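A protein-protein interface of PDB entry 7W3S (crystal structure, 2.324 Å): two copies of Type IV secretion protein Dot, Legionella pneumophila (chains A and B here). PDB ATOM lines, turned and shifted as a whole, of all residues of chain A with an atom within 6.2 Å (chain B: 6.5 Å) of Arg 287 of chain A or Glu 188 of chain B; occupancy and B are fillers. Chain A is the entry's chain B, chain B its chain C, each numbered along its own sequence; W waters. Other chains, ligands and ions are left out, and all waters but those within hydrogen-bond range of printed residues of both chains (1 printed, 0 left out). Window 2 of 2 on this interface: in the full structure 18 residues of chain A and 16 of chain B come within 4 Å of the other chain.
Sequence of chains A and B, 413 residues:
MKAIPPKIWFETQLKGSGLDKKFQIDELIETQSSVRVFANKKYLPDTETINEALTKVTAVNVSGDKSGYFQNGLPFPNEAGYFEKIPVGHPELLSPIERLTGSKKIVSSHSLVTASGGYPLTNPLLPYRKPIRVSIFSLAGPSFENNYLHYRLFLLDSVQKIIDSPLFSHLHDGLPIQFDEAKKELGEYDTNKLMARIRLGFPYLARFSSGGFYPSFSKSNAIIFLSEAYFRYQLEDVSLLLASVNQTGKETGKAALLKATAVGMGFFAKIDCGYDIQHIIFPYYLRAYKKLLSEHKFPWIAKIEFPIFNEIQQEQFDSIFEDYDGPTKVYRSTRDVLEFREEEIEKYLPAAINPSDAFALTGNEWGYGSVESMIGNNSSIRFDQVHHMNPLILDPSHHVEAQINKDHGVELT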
ATOM      1  N   PHE A 231     -13.979  -8.470 -11.995  1.00  0.00           N
ATOM      2  CA  PHE A 231     -12.750  -9.084 -11.494  1.00  0.00           C
ATOM      3  C   PHE A 231     -11.597  -8.088 -11.511  1.00  0.00           C
ATOM      4  O   PHE A 231     -10.816  -8.012 -10.551  1.00  0.00           O
ATOM      5  CB  PHE A 231     -12.410 -10.316 -12.328  1.00  0.00           C
ATOM      6  CG  PHE A 231     -11.162 -11.027 -11.891  1.00  0.00           C
ATOM      7  CD1 PHE A 231     -11.050 -11.529 -10.610  1.00  0.00           C
ATOM      8  CD2 PHE A 231     -10.114 -11.218 -12.773  1.00  0.00           C
ATOM      9  CE1 PHE A 231      -9.906 -12.182 -10.204  1.00  0.00           C
ATOM     10  CE2 PHE A 231      -8.972 -11.882 -12.379  1.00  0.00           C
ATOM     11  CZ  PHE A 231      -8.862 -12.359 -11.091  1.00  0.00           C
ATOM     12  N   LEU A 235      -9.414  -6.628  -8.325  1.00  0.00           N
ATOM     13  CA  LEU A 235      -7.957  -6.649  -8.225  1.00  0.00           C
ATOM     14  C   LEU A 235      -7.401  -5.294  -7.795  1.00  0.00           C
ATOM     15  O   LEU A 235      -6.351  -5.247  -7.140  1.00  0.00           O
ATOM     16  CB  LEU A 235      -7.322  -7.088  -9.548  1.00  0.00           C
ATOM     17  CG  LEU A 235      -7.611  -8.533  -9.979  1.00  0.00           C
ATOM     18  CD1 LEU A 235      -7.299  -8.731 -11.456  1.00  0.00           C
ATOM     19  CD2 LEU A 235      -6.841  -9.543  -9.133  1.00  0.00           C
ATOM     20  N   PHE A 282     -18.949 -13.383  -5.284  1.00  0.00           N
ATOM     21  CA  PHE A 282     -17.995 -13.886  -4.295  1.00  0.00           C
ATOM     22  C   PHE A 282     -16.798 -14.616  -4.900  1.00  0.00           C
ATOM     23  O   PHE A 282     -15.663 -14.338  -4.463  1.00  0.00           O
ATOM     24  CB  PHE A 282     -18.731 -14.787  -3.293  1.00  0.00           C
ATOM     25  CG  PHE A 282     -17.929 -15.105  -2.062  1.00  0.00           C
ATOM     26  CD1 PHE A 282     -17.390 -14.078  -1.281  1.00  0.00           C
ATOM     27  CD2 PHE A 282     -17.723 -16.428  -1.679  1.00  0.00           C
ATOM     28  CE1 PHE A 282     -16.642 -14.366  -0.133  1.00  0.00           C
ATOM     29  CE2 PHE A 282     -16.984 -16.732  -0.534  1.00  0.00           C
ATOM     30  CZ  PHE A 282     -16.431 -15.692   0.243  1.00  0.00           C
ATOM     31  N   PRO A 283     -16.952 -15.522  -5.885  1.00  0.00           N
ATOM     32  CA  PRO A 283     -15.756 -16.162  -6.469  1.00  0.00           C
ATOM     33  C   PRO A 283     -14.747 -15.178  -7.042  1.00  0.00           C
ATOM     34  O   PRO A 283     -13.540 -15.445  -6.994  1.00  0.00           O
ATOM     35  CB  PRO A 283     -16.340 -17.071  -7.566  1.00  0.00           C
ATOM     36  CG  PRO A 283     -17.757 -17.324  -7.158  1.00  0.00           C
ATOM     37  CD  PRO A 283     -18.203 -16.073  -6.452  1.00  0.00           C
ATOM     38  N   TYR A 284     -15.200 -14.054  -7.594  1.00  0.00           N
ATOM     39  CA  TYR A 284     -14.265 -13.059  -8.111  1.00  0.00           C
ATOM     40  C   TYR A 284     -13.563 -12.313  -6.981  1.00  0.00           C
ATOM     41  O   TYR A 284     -12.382 -11.965  -7.107  1.00  0.00           O
ATOM     42  CB  TYR A 284     -14.998 -12.116  -9.062  1.00  0.00           C
ATOM     43  CG  TYR A 284     -15.514 -12.894 -10.238  1.00  0.00           C
ATOM     44  CD1 TYR A 284     -14.629 -13.433 -11.155  1.00  0.00           C
ATOM     45  CD2 TYR A 284     -16.870 -13.162 -10.397  1.00  0.00           C
ATOM     46  CE1 TYR A 284     -15.068 -14.193 -12.214  1.00  0.00           C
ATOM     47  CE2 TYR A 284     -17.324 -13.937 -11.466  1.00  0.00           C
ATOM     48  CZ  TYR A 284     -16.403 -14.444 -12.364  1.00  0.00           C
ATOM     49  OH  TYR A 284     -16.784 -15.205 -13.429  1.00  0.00           O
ATOM     50  N   TYR A 285     -14.259 -12.090  -5.864  1.00  0.00           N
ATOM     51  CA  TYR A 285     -13.584 -11.617  -4.662  1.00  0.00           C
ATOM     52  C   TYR A 285     -12.450 -12.566  -4.278  1.00  0.00           C
ATOM     53  O   TYR A 285     -11.307 -12.136  -4.086  1.00  0.00           O
ATOM     54  CB  TYR A 285     -14.593 -11.463  -3.520  1.00  0.00           C
ATOM     55  CG  TYR A 285     -14.036 -10.842  -2.261  1.00  0.00           C
ATOM     56  CD1 TYR A 285     -13.438  -9.580  -2.278  1.00  0.00           C
ATOM     57  CD2 TYR A 285     -14.106 -11.515  -1.047  1.00  0.00           C
ATOM     58  CE1 TYR A 285     -12.912  -9.005  -1.104  1.00  0.00           C
ATOM     59  CE2 TYR A 285     -13.575 -10.953   0.133  1.00  0.00           C
ATOM     60  CZ  TYR A 285     -12.983  -9.708   0.101  1.00  0.00           C
ATOM     61  OH  TYR A 285     -12.478  -9.176   1.279  1.00  0.00           O
ATOM     62  N   LEU A 286     -12.736 -13.875  -4.218  1.00  0.00           N
ATOM     63  CA  LEU A 286     -11.724 -14.827  -3.756  1.00  0.00           C
ATOM     64  C   LEU A 286     -10.590 -14.988  -4.774  1.00  0.00           C
ATOM     65  O   LEU A 286      -9.418 -15.081  -4.393  1.00  0.00           O
ATOM     66  CB  LEU A 286     -12.379 -16.173  -3.439  1.00  0.00           C
ATOM     67  CG  LEU A 286     -13.441 -16.119  -2.335  1.00  0.00           C
ATOM     68  CD1 LEU A 286     -14.114 -17.473  -2.161  1.00  0.00           C
ATOM     69  CD2 LEU A 286     -12.840 -15.637  -1.011  1.00  0.00           C
ATOM     70  N   ARG A 287     -10.915 -15.008  -6.067  1.00  0.00           N
ATOM     71  CA  ARG A 287      -9.876 -15.113  -7.089  1.00  0.00           C
ATOM     72  C   ARG A 287      -8.951 -13.899  -7.097  1.00  0.00           C
ATOM     73  O   ARG A 287      -7.776 -14.039  -7.445  1.00  0.00           O
ATOM     74  CB  ARG A 287     -10.508 -15.316  -8.478  1.00  0.00           C
ATOM     75  CG  ARG A 287     -11.225 -16.644  -8.608  1.00  0.00           C
ATOM     76  CD  ARG A 287     -11.537 -17.035 -10.042  1.00  0.00           C
ATOM     77  NE  ARG A 287     -11.957 -18.436 -10.112  1.00  0.00           N
ATOM     78  CZ  ARG A 287     -11.133 -19.484  -9.966  1.00  0.00           C
ATOM     79  NH1 ARG A 287      -9.833 -19.294  -9.737  1.00  0.00           N
ATOM     80  NH2 ARG A 287     -11.604 -20.730 -10.046  1.00  0.00           N
ATOM     81  N   ALA A 288      -9.449 -12.706  -6.735  1.00  0.00           N
ATOM     82  CA  ALA A 288      -8.565 -11.539  -6.661  1.00  0.00           C
ATOM     83  C   ALA A 288      -7.457 -11.757  -5.637  1.00  0.00           C
ATOM     84  O   ALA A 288      -6.283 -11.477  -5.906  1.00  0.00           O
ATOM     85  CB  ALA A 288      -9.350 -10.272  -6.326  1.00  0.00           C
ATOM     86  N   TYR A 289      -7.819 -12.257  -4.448  1.00  0.00           N
ATOM     87  CA  TYR A 289      -6.817 -12.634  -3.451  1.00  0.00           C
ATOM     88  C   TYR A 289      -5.889 -13.708  -3.992  1.00  0.00           C
ATOM     89  O   TYR A 289      -4.661 -13.570  -3.926  1.00  0.00           O
ATOM     90  CB  TYR A 289      -7.495 -13.139  -2.177  1.00  0.00           C
ATOM     91  CG  TYR A 289      -8.083 -12.060  -1.300  1.00  0.00           C
ATOM     92  CD1 TYR A 289      -7.324 -11.452  -0.313  1.00  0.00           C
ATOM     93  CD2 TYR A 289      -9.402 -11.654  -1.454  1.00  0.00           C
ATOM     94  CE1 TYR A 289      -7.866 -10.477   0.502  1.00  0.00           C
ATOM     95  CE2 TYR A 289      -9.948 -10.657  -0.655  1.00  0.00           C
ATOM     96  CZ  TYR A 289      -9.177 -10.082   0.331  1.00  0.00           C
ATOM     97  OH  TYR A 289      -9.720  -9.102   1.140  1.00  0.00           O
ATOM     98  N   LYS A 290      -6.466 -14.788  -4.543  1.00  0.00           N
ATOM     99  CA  LYS A 290      -5.662 -15.932  -4.970  1.00  0.00           C
ATOM    100  C   LYS A 290      -4.643 -15.527  -6.028  1.00  0.00           C
ATOM    101  O   LYS A 290      -3.479 -15.948  -5.972  1.00  0.00           O
ATOM    102  CB  LYS A 290      -6.564 -17.055  -5.494  1.00  0.00           C
ATOM    103  CG  LYS A 290      -5.809 -18.295  -5.961  1.00  0.00           C
ATOM    104  CD  LYS A 290      -6.673 -19.185  -6.855  1.00  0.00           C
ATOM    105  CE  LYS A 290      -5.961 -20.505  -7.161  1.00  0.00           C
ATOM    106  NZ  LYS A 290      -6.754 -21.440  -8.024  1.00  0.00           N
ATOM    107  N   LYS A 291      -5.060 -14.705  -6.995  1.00  0.00           N
ATOM    108  CA  LYS A 291      -4.129 -14.174  -7.982  1.00  0.00           C
ATOM    109  C   LYS A 291      -3.042 -13.335  -7.311  1.00  0.00           C
ATOM    110  O   LYS A 291      -1.845 -13.624  -7.437  1.00  0.00           O
ATOM    111  CB  LYS A 291      -4.893 -13.346  -9.025  1.00  0.00           C
ATOM    112  CG  LYS A 291      -4.019 -12.767 -10.142  1.00  0.00           C
ATOM    113  CD  LYS A 291      -4.814 -11.859 -11.071  1.00  0.00           C
ATOM    114  CE  LYS A 291      -4.224 -11.817 -12.475  1.00  0.00           C
ATOM    115  NZ  LYS A 291      -2.739 -11.772 -12.467  1.00  0.00           N
ATOM    116  N   LEU A 292      -3.446 -12.295  -6.576  1.00  0.00           N
ATOM    117  CA  LEU A 292      -2.483 -11.338  -6.034  1.00  0.00           C
ATOM    118  C   LEU A 292      -1.536 -11.990  -5.043  1.00  0.00           C
ATOM    119  O   LEU A 292      -0.326 -11.743  -5.082  1.00  0.00           O
ATOM    120  CB  LEU A 292      -3.213 -10.165  -5.381  1.00  0.00           C
ATOM    121  CG  LEU A 292      -3.907  -9.288  -6.417  1.00  0.00           C
ATOM    122  CD1 LEU A 292      -4.834  -8.293  -5.755  1.00  0.00           C
ATOM    123  CD2 LEU A 292      -2.867  -8.606  -7.270  1.00  0.00           C
ATOM    124  N   GLU A 315     -17.896 -23.765   0.054  1.00  0.00           N
ATOM    125  CA  GLU A 315     -17.450 -24.697  -0.973  1.00  0.00           C
ATOM    126  C   GLU A 315     -16.847 -23.967  -2.167  1.00  0.00           C
ATOM    127  O   GLU A 315     -15.967 -24.510  -2.843  1.00  0.00           O
ATOM    128  CB  GLU A 315     -18.608 -25.610  -1.398  1.00  0.00           C
ATOM    129  CG  GLU A 315     -18.622 -26.921  -0.609  1.00  0.00           C
ATOM    130  CD  GLU A 315     -19.784 -27.866  -0.948  1.00  0.00           C
ATOM    131  OE1 GLU A 315     -20.277 -27.883  -2.109  1.00  0.00           O
ATOM    132  OE2 GLU A 315     -20.200 -28.603  -0.026  1.00  0.00           O
ATOM    133  N   GLN A 316     -17.286 -22.733  -2.436  1.00  0.00           N
ATOM    134  CA  GLN A 316     -16.594 -21.939  -3.449  1.00  0.00           C
ATOM    135  C   GLN A 316     -15.168 -21.631  -3.006  1.00  0.00           C
ATOM    136  O   GLN A 316     -14.225 -21.717  -3.806  1.00  0.00           O
ATOM    137  CB  GLN A 316     -17.363 -20.651  -3.727  1.00  0.00           C
ATOM    138  CG  GLN A 316     -18.645 -20.863  -4.491  1.00  0.00           C
ATOM    139  CD  GLN A 316     -19.535 -19.632  -4.505  1.00  0.00           C
ATOM    140  OE1 GLN A 316     -19.381 -18.727  -3.687  1.00  0.00           O
ATOM    141  NE2 GLN A 316     -20.470 -19.589  -5.449  1.00  0.00           N
ATOM    142  N   SER A 319     -12.918 -24.845  -3.230  1.00  0.00           N
ATOM    143  CA  SER A 319     -12.595 -25.154  -4.619  1.00  0.00           C
ATOM    144  C   SER A 319     -11.647 -24.119  -5.222  1.00  0.00           C
ATOM    145  O   SER A 319     -10.731 -24.469  -5.974  1.00  0.00           O
ATOM    146  CB  SER A 319     -13.887 -25.251  -5.439  1.00  0.00           C
ATOM    147  OG  SER A 319     -13.609 -25.278  -6.828  1.00  0.00           O
ATOM    148  N   ILE A 320     -11.847 -22.837  -4.922  1.00  0.00           N
ATOM    149  CA  ILE A 320     -10.980 -21.836  -5.529  1.00  0.00           C
ATOM    150  C   ILE A 320      -9.557 -21.920  -4.964  1.00  0.00           C
ATOM    151  O   ILE A 320      -8.587 -21.661  -5.687  1.00  0.00           O
ATOM    152  CB  ILE A 320     -11.613 -20.442  -5.365  1.00  0.00           C
ATOM    153  CG1 ILE A 320     -12.687 -20.236  -6.434  1.00  0.00           C
ATOM    154  CG2 ILE A 320     -10.554 -19.319  -5.402  1.00  0.00           C
ATOM    155  CD1 ILE A 320     -13.791 -19.296  -6.020  1.00  0.00           C
ATOM    156  N   PHE A 321      -9.395 -22.327  -3.700  1.00  0.00           N
ATOM    157  CA  PHE A 321      -8.087 -22.295  -3.052  1.00  0.00           C
ATOM    158  C   PHE A 321      -7.410 -23.656  -2.955  1.00  0.00           C
ATOM    159  O   PHE A 321      -6.298 -23.734  -2.413  1.00  0.00           O
ATOM    160  CB  PHE A 321      -8.193 -21.666  -1.652  1.00  0.00           C
ATOM    161  CG  PHE A 321      -8.189 -20.159  -1.675  1.00  0.00           C
ATOM    162  CD1 PHE A 321      -7.000 -19.458  -1.812  1.00  0.00           C
ATOM    163  CD2 PHE A 321      -9.381 -19.445  -1.593  1.00  0.00           C
ATOM    164  CE1 PHE A 321      -6.997 -18.067  -1.861  1.00  0.00           C
ATOM    165  CE2 PHE A 321      -9.387 -18.068  -1.646  1.00  0.00           C
ATOM    166  CZ  PHE A 321      -8.195 -17.375  -1.778  1.00  0.00           C
ATOM    167  N   LYS B 183     -16.787 -33.153 -11.624  1.00  0.00           N
ATOM    168  CA  LYS B 183     -16.796 -32.144 -10.561  1.00  0.00           C
ATOM    169  C   LYS B 183     -15.633 -31.168 -10.714  1.00  0.00           C
ATOM    170  O   LYS B 183     -15.791 -29.958 -10.503  1.00  0.00           O
ATOM    171  CB  LYS B 183     -16.746 -32.819  -9.186  1.00  0.00           C
ATOM    172  CG  LYS B 183     -18.109 -33.233  -8.637  1.00  0.00           C
ATOM    173  CD  LYS B 183     -18.099 -33.392  -7.122  1.00  0.00           C
ATOM    174  CE  LYS B 183     -17.814 -34.835  -6.717  1.00  0.00           C
ATOM    175  NZ  LYS B 183     -17.698 -34.974  -5.240  1.00  0.00           N
ATOM    176  N   LYS B 184     -14.459 -31.678 -11.100  1.00  0.00           N
ATOM    177  CA  LYS B 184     -13.280 -30.829 -11.235  1.00  0.00           C
ATOM    178  C   LYS B 184     -13.411 -29.876 -12.417  1.00  0.00           C
ATOM    179  O   LYS B 184     -13.059 -28.696 -12.305  1.00  0.00           O
ATOM    180  CB  LYS B 184     -12.025 -31.695 -11.385  1.00  0.00           C
ATOM    181  CG  LYS B 184     -11.274 -31.924 -10.089  1.00  0.00           C
ATOM    182  CD  LYS B 184      -9.809 -32.259 -10.355  1.00  0.00           C
ATOM    183  CE  LYS B 184      -8.941 -31.005 -10.361  1.00  0.00           C
ATOM    184  NZ  LYS B 184      -7.487 -31.336 -10.448  1.00  0.00           N
ATOM    185  N   LEU B 186     -16.016 -28.585 -13.600  1.00  0.00           N
ATOM    186  CA  LEU B 186     -16.960 -27.523 -13.267  1.00  0.00           C
ATOM    187  C   LEU B 186     -16.346 -26.502 -12.309  1.00  0.00           C
ATOM    188  O   LEU B 186     -16.541 -25.289 -12.475  1.00  0.00           O
ATOM    189  CB  LEU B 186     -18.228 -28.124 -12.666  1.00  0.00           C
ATOM    190  CG  LEU B 186     -19.026 -29.059 -13.579  1.00  0.00           C
ATOM    191  CD1 LEU B 186     -20.376 -29.344 -12.957  1.00  0.00           C
ATOM    192  CD2 LEU B 186     -19.181 -28.481 -14.971  1.00  0.00           C
ATOM    193  N   GLY B 187     -15.611 -26.969 -11.300  1.00  0.00           N
ATOM    194  CA  GLY B 187     -15.006 -26.053 -10.339  1.00  0.00           C
ATOM    195  C   GLY B 187     -16.043 -25.523  -9.369  1.00  0.00           C
ATOM    196  O   GLY B 187     -16.802 -26.295  -8.766  1.00  0.00           O
ATOM    197  N   GLU B 188     -16.083 -24.197  -9.212  1.00  0.00           N
ATOM    198  CA  GLU B 188     -17.053 -23.555  -8.334  1.00  0.00           C
ATOM    199  C   GLU B 188     -18.379 -23.270  -9.026  1.00  0.00           C
ATOM    200  O   GLU B 188     -19.342 -22.891  -8.347  1.00  0.00           O
ATOM    201  CB  GLU B 188     -16.485 -22.245  -7.757  1.00  0.00           C
ATOM    202  CG  GLU B 188     -16.363 -21.106  -8.773  1.00  0.00           C
ATOM    203  CD  GLU B 188     -14.953 -20.977  -9.349  1.00  0.00           C
ATOM    204  OE1 GLU B 188     -14.539 -19.835  -9.667  1.00  0.00           O
ATOM    205  OE2 GLU B 188     -14.258 -22.019  -9.476  1.00  0.00           O
ATOM    206  N   TYR B 189     -18.450 -23.448 -10.347  1.00  0.00           N
ATOM    207  CA  TYR B 189     -19.673 -23.222 -11.105  1.00  0.00           C
ATOM    208  C   TYR B 189     -20.473 -24.518 -11.246  1.00  0.00           C
ATOM    209  O   TYR B 189     -20.021 -25.610 -10.901  1.00  0.00           O
ATOM    210  CB  TYR B 189     -19.353 -22.625 -12.479  1.00  0.00           C
ATOM    211  CG  TYR B 189     -18.692 -21.275 -12.365  1.00  0.00           C
ATOM    212  CD1 TYR B 189     -19.385 -20.188 -11.841  1.00  0.00           C
ATOM    213  CD2 TYR B 189     -17.363 -21.092 -12.740  1.00  0.00           C
ATOM    214  CE1 TYR B 189     -18.782 -18.951 -11.708  1.00  0.00           C
ATOM    215  CE2 TYR B 189     -16.752 -19.850 -12.616  1.00  0.00           C
ATOM    216  CZ  TYR B 189     -17.467 -18.786 -12.093  1.00  0.00           C
ATOM    217  OH  TYR B 189     -16.877 -17.552 -11.957  1.00  0.00           O
ATOM    218  N   ASP B 190     -21.690 -24.382 -11.756  1.00  0.00           N
ATOM    219  CA  ASP B 190     -22.600 -25.507 -11.858  1.00  0.00           C
ATOM    220  C   ASP B 190     -22.856 -25.942 -13.296  1.00  0.00           C
ATOM    221  O   ASP B 190     -23.508 -26.969 -13.505  1.00  0.00           O
ATOM    222  CB  ASP B 190     -23.922 -25.165 -11.161  1.00  0.00           C
ATOM    223  CG  ASP B 190     -23.775 -25.050  -9.651  1.00  0.00           C
ATOM    224  OD1 ASP B 190     -22.833 -25.652  -9.093  1.00  0.00           O
ATOM    225  OD2 ASP B 190     -24.602 -24.358  -9.017  1.00  0.00           O
ATOM    226  N   ARG B 197     -24.942 -29.463 -13.189  1.00  0.00           N
ATOM    227  CA  ARG B 197     -25.634 -30.025 -12.044  1.00  0.00           C
ATOM    228  C   ARG B 197     -27.117 -29.704 -12.166  1.00  0.00           C
ATOM    229  O   ARG B 197     -27.529 -28.837 -12.943  1.00  0.00           O
ATOM    230  CB  ARG B 197     -25.060 -29.481 -10.729  1.00  0.00           C
ATOM    231  CG  ARG B 197     -23.952 -30.352 -10.118  1.00  0.00           C
ATOM    232  CD  ARG B 197     -23.309 -29.742  -8.855  1.00  0.00           C
ATOM    233  NE  ARG B 197     -22.298 -28.751  -9.208  1.00  0.00           N
ATOM    234  CZ  ARG B 197     -21.010 -29.019  -9.383  1.00  0.00           C
ATOM    235  NH1 ARG B 197     -20.181 -28.048  -9.719  1.00  0.00           N
ATOM    236  NH2 ARG B 197     -20.550 -30.252  -9.239  1.00  0.00           N
ATOM    237  N   TYR B 204     -29.360 -28.582  -5.005  1.00  0.00           N
ATOM    238  CA  TYR B 204     -29.115 -29.548  -6.062  1.00  0.00           C
ATOM    239  C   TYR B 204     -29.782 -30.879  -5.741  1.00  0.00           C
ATOM    240  O   TYR B 204     -30.209 -31.137  -4.616  1.00  0.00           O
ATOM    241  CB  TYR B 204     -27.613 -29.772  -6.255  1.00  0.00           C
ATOM    242  CG  TYR B 204     -26.793 -28.513  -6.310  1.00  0.00           C
ATOM    243  CD1 TYR B 204     -26.833 -27.687  -7.422  1.00  0.00           C
ATOM    244  CD2 TYR B 204     -25.959 -28.161  -5.261  1.00  0.00           C
ATOM    245  CE1 TYR B 204     -26.074 -26.530  -7.489  1.00  0.00           C
ATOM    246  CE2 TYR B 204     -25.185 -27.001  -5.314  1.00  0.00           C
ATOM    247  CZ  TYR B 204     -25.246 -26.190  -6.430  1.00  0.00           C
ATOM    248  OH  TYR B 204     -24.486 -25.037  -6.488  1.00  0.00           O
ATOM    249  N   LYS B 219     -21.963 -29.606  -3.129  1.00  0.00           N
ATOM    250  CA  LYS B 219     -21.701 -30.061  -4.488  1.00  0.00           C
ATOM    251  C   LYS B 219     -21.062 -31.453  -4.558  1.00  0.00           C
ATOM    252  O   LYS B 219     -20.717 -31.904  -5.654  1.00  0.00           O
ATOM    253  CB  LYS B 219     -20.819 -29.037  -5.214  1.00  0.00           C
ATOM    254  CG  LYS B 219     -21.608 -27.855  -5.755  1.00  0.00           C
ATOM    255  CD  LYS B 219     -20.780 -26.572  -5.830  1.00  0.00           C
ATOM    256  CE  LYS B 219     -21.582 -25.345  -5.345  1.00  0.00           C
ATOM    257  NZ  LYS B 219     -22.143 -25.545  -3.952  1.00  0.00           N
HETATM  258  O   HOH W   1     -21.979 -22.326  -6.731  1.00  0.00           O
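The guanidinium group (NE) of Arg 287 of chain A is in salt-bridge range of the side-chain carboxylate (OE1) of Glu 188 of chain B, 3.0 Å away.
NZ of Lys 219 of chain B lies within salt-bridge range of OE1 of Glu 315 of chain A.
OH of Tyr 189 of chain B is in hydrogen-bond range of OH of Tyr 284 of chain A.
The side-chain hydroxyl (OH) of Tyr 204 of chain B sits close to the side-chain amino group (NZ) of Lys 219 of chain B (3.5 Å).
The backbone carbonyl oxygen of Ile 320 of chain A lies within hydrogen-bond range of the side-chain amino group of Lys 290 of chain A (3.0 Å).
The guanidinium group of Arg 197 of chain B lies within hydrogen-bond range of the backbone carbonyl oxygen of Tyr 189 of chain B.
Pro 283 of chain A touches Glu 188 of chain B.
OG of Ser 319 of chain A touches C of Gly 187 of chain B, at 3.5 Å.
OG of Ser 319 of chain A touches N of Glu 188 of chain B (3.6 Å).
Ile 320 of chain A touches Glu 188 of chain B (CG1 to OE1, 3.7 Å).
Of chain B, only Glu 188 (3.0 Å) comes within 4 Å of Arg 287 of chain A.
Of the printed residues of chain B, Tyr 284 of chain A touches Tyr 189.
Of the printed residues of chain B, Ile 320 of chain A touches Glu 188.
Of the printed residues of chain A, Tyr 189 of chain B touches Tyr 284.
The nearest printed residue of chain A that does not touch Tyr 189 of chain B is Pro 283 of chain A (4.4 Å).
Of the 18 printed residues of chain A, 6 touch a printed residue of chain B.
Printed residues of chain A that touch a printed residue of chain B: Pro 283, Tyr 284, Arg 287, Glu 315, Ser 319 and Ile 320.
Hydrophobic or aromatic side chains of chain A that line the printed part of chain B: Pro 283, Tyr 284 and Ile 320.
Of the 10 printed residues of chain B, 4 touch a printed residue of chain A.
No position is printed for both chains.
Of the 7 pairs that touch across the chains among the printed residues, none has its exchanged pair printed and touching as well.
Water W1 lies within hydrogen-bond range of the backbone carbonyl oxygen (O) of Glu 188 of chain B (3.1 Å) and the side-chain amide nitrogen (NE2) of Gln 316 of chain A (3.4 Å).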
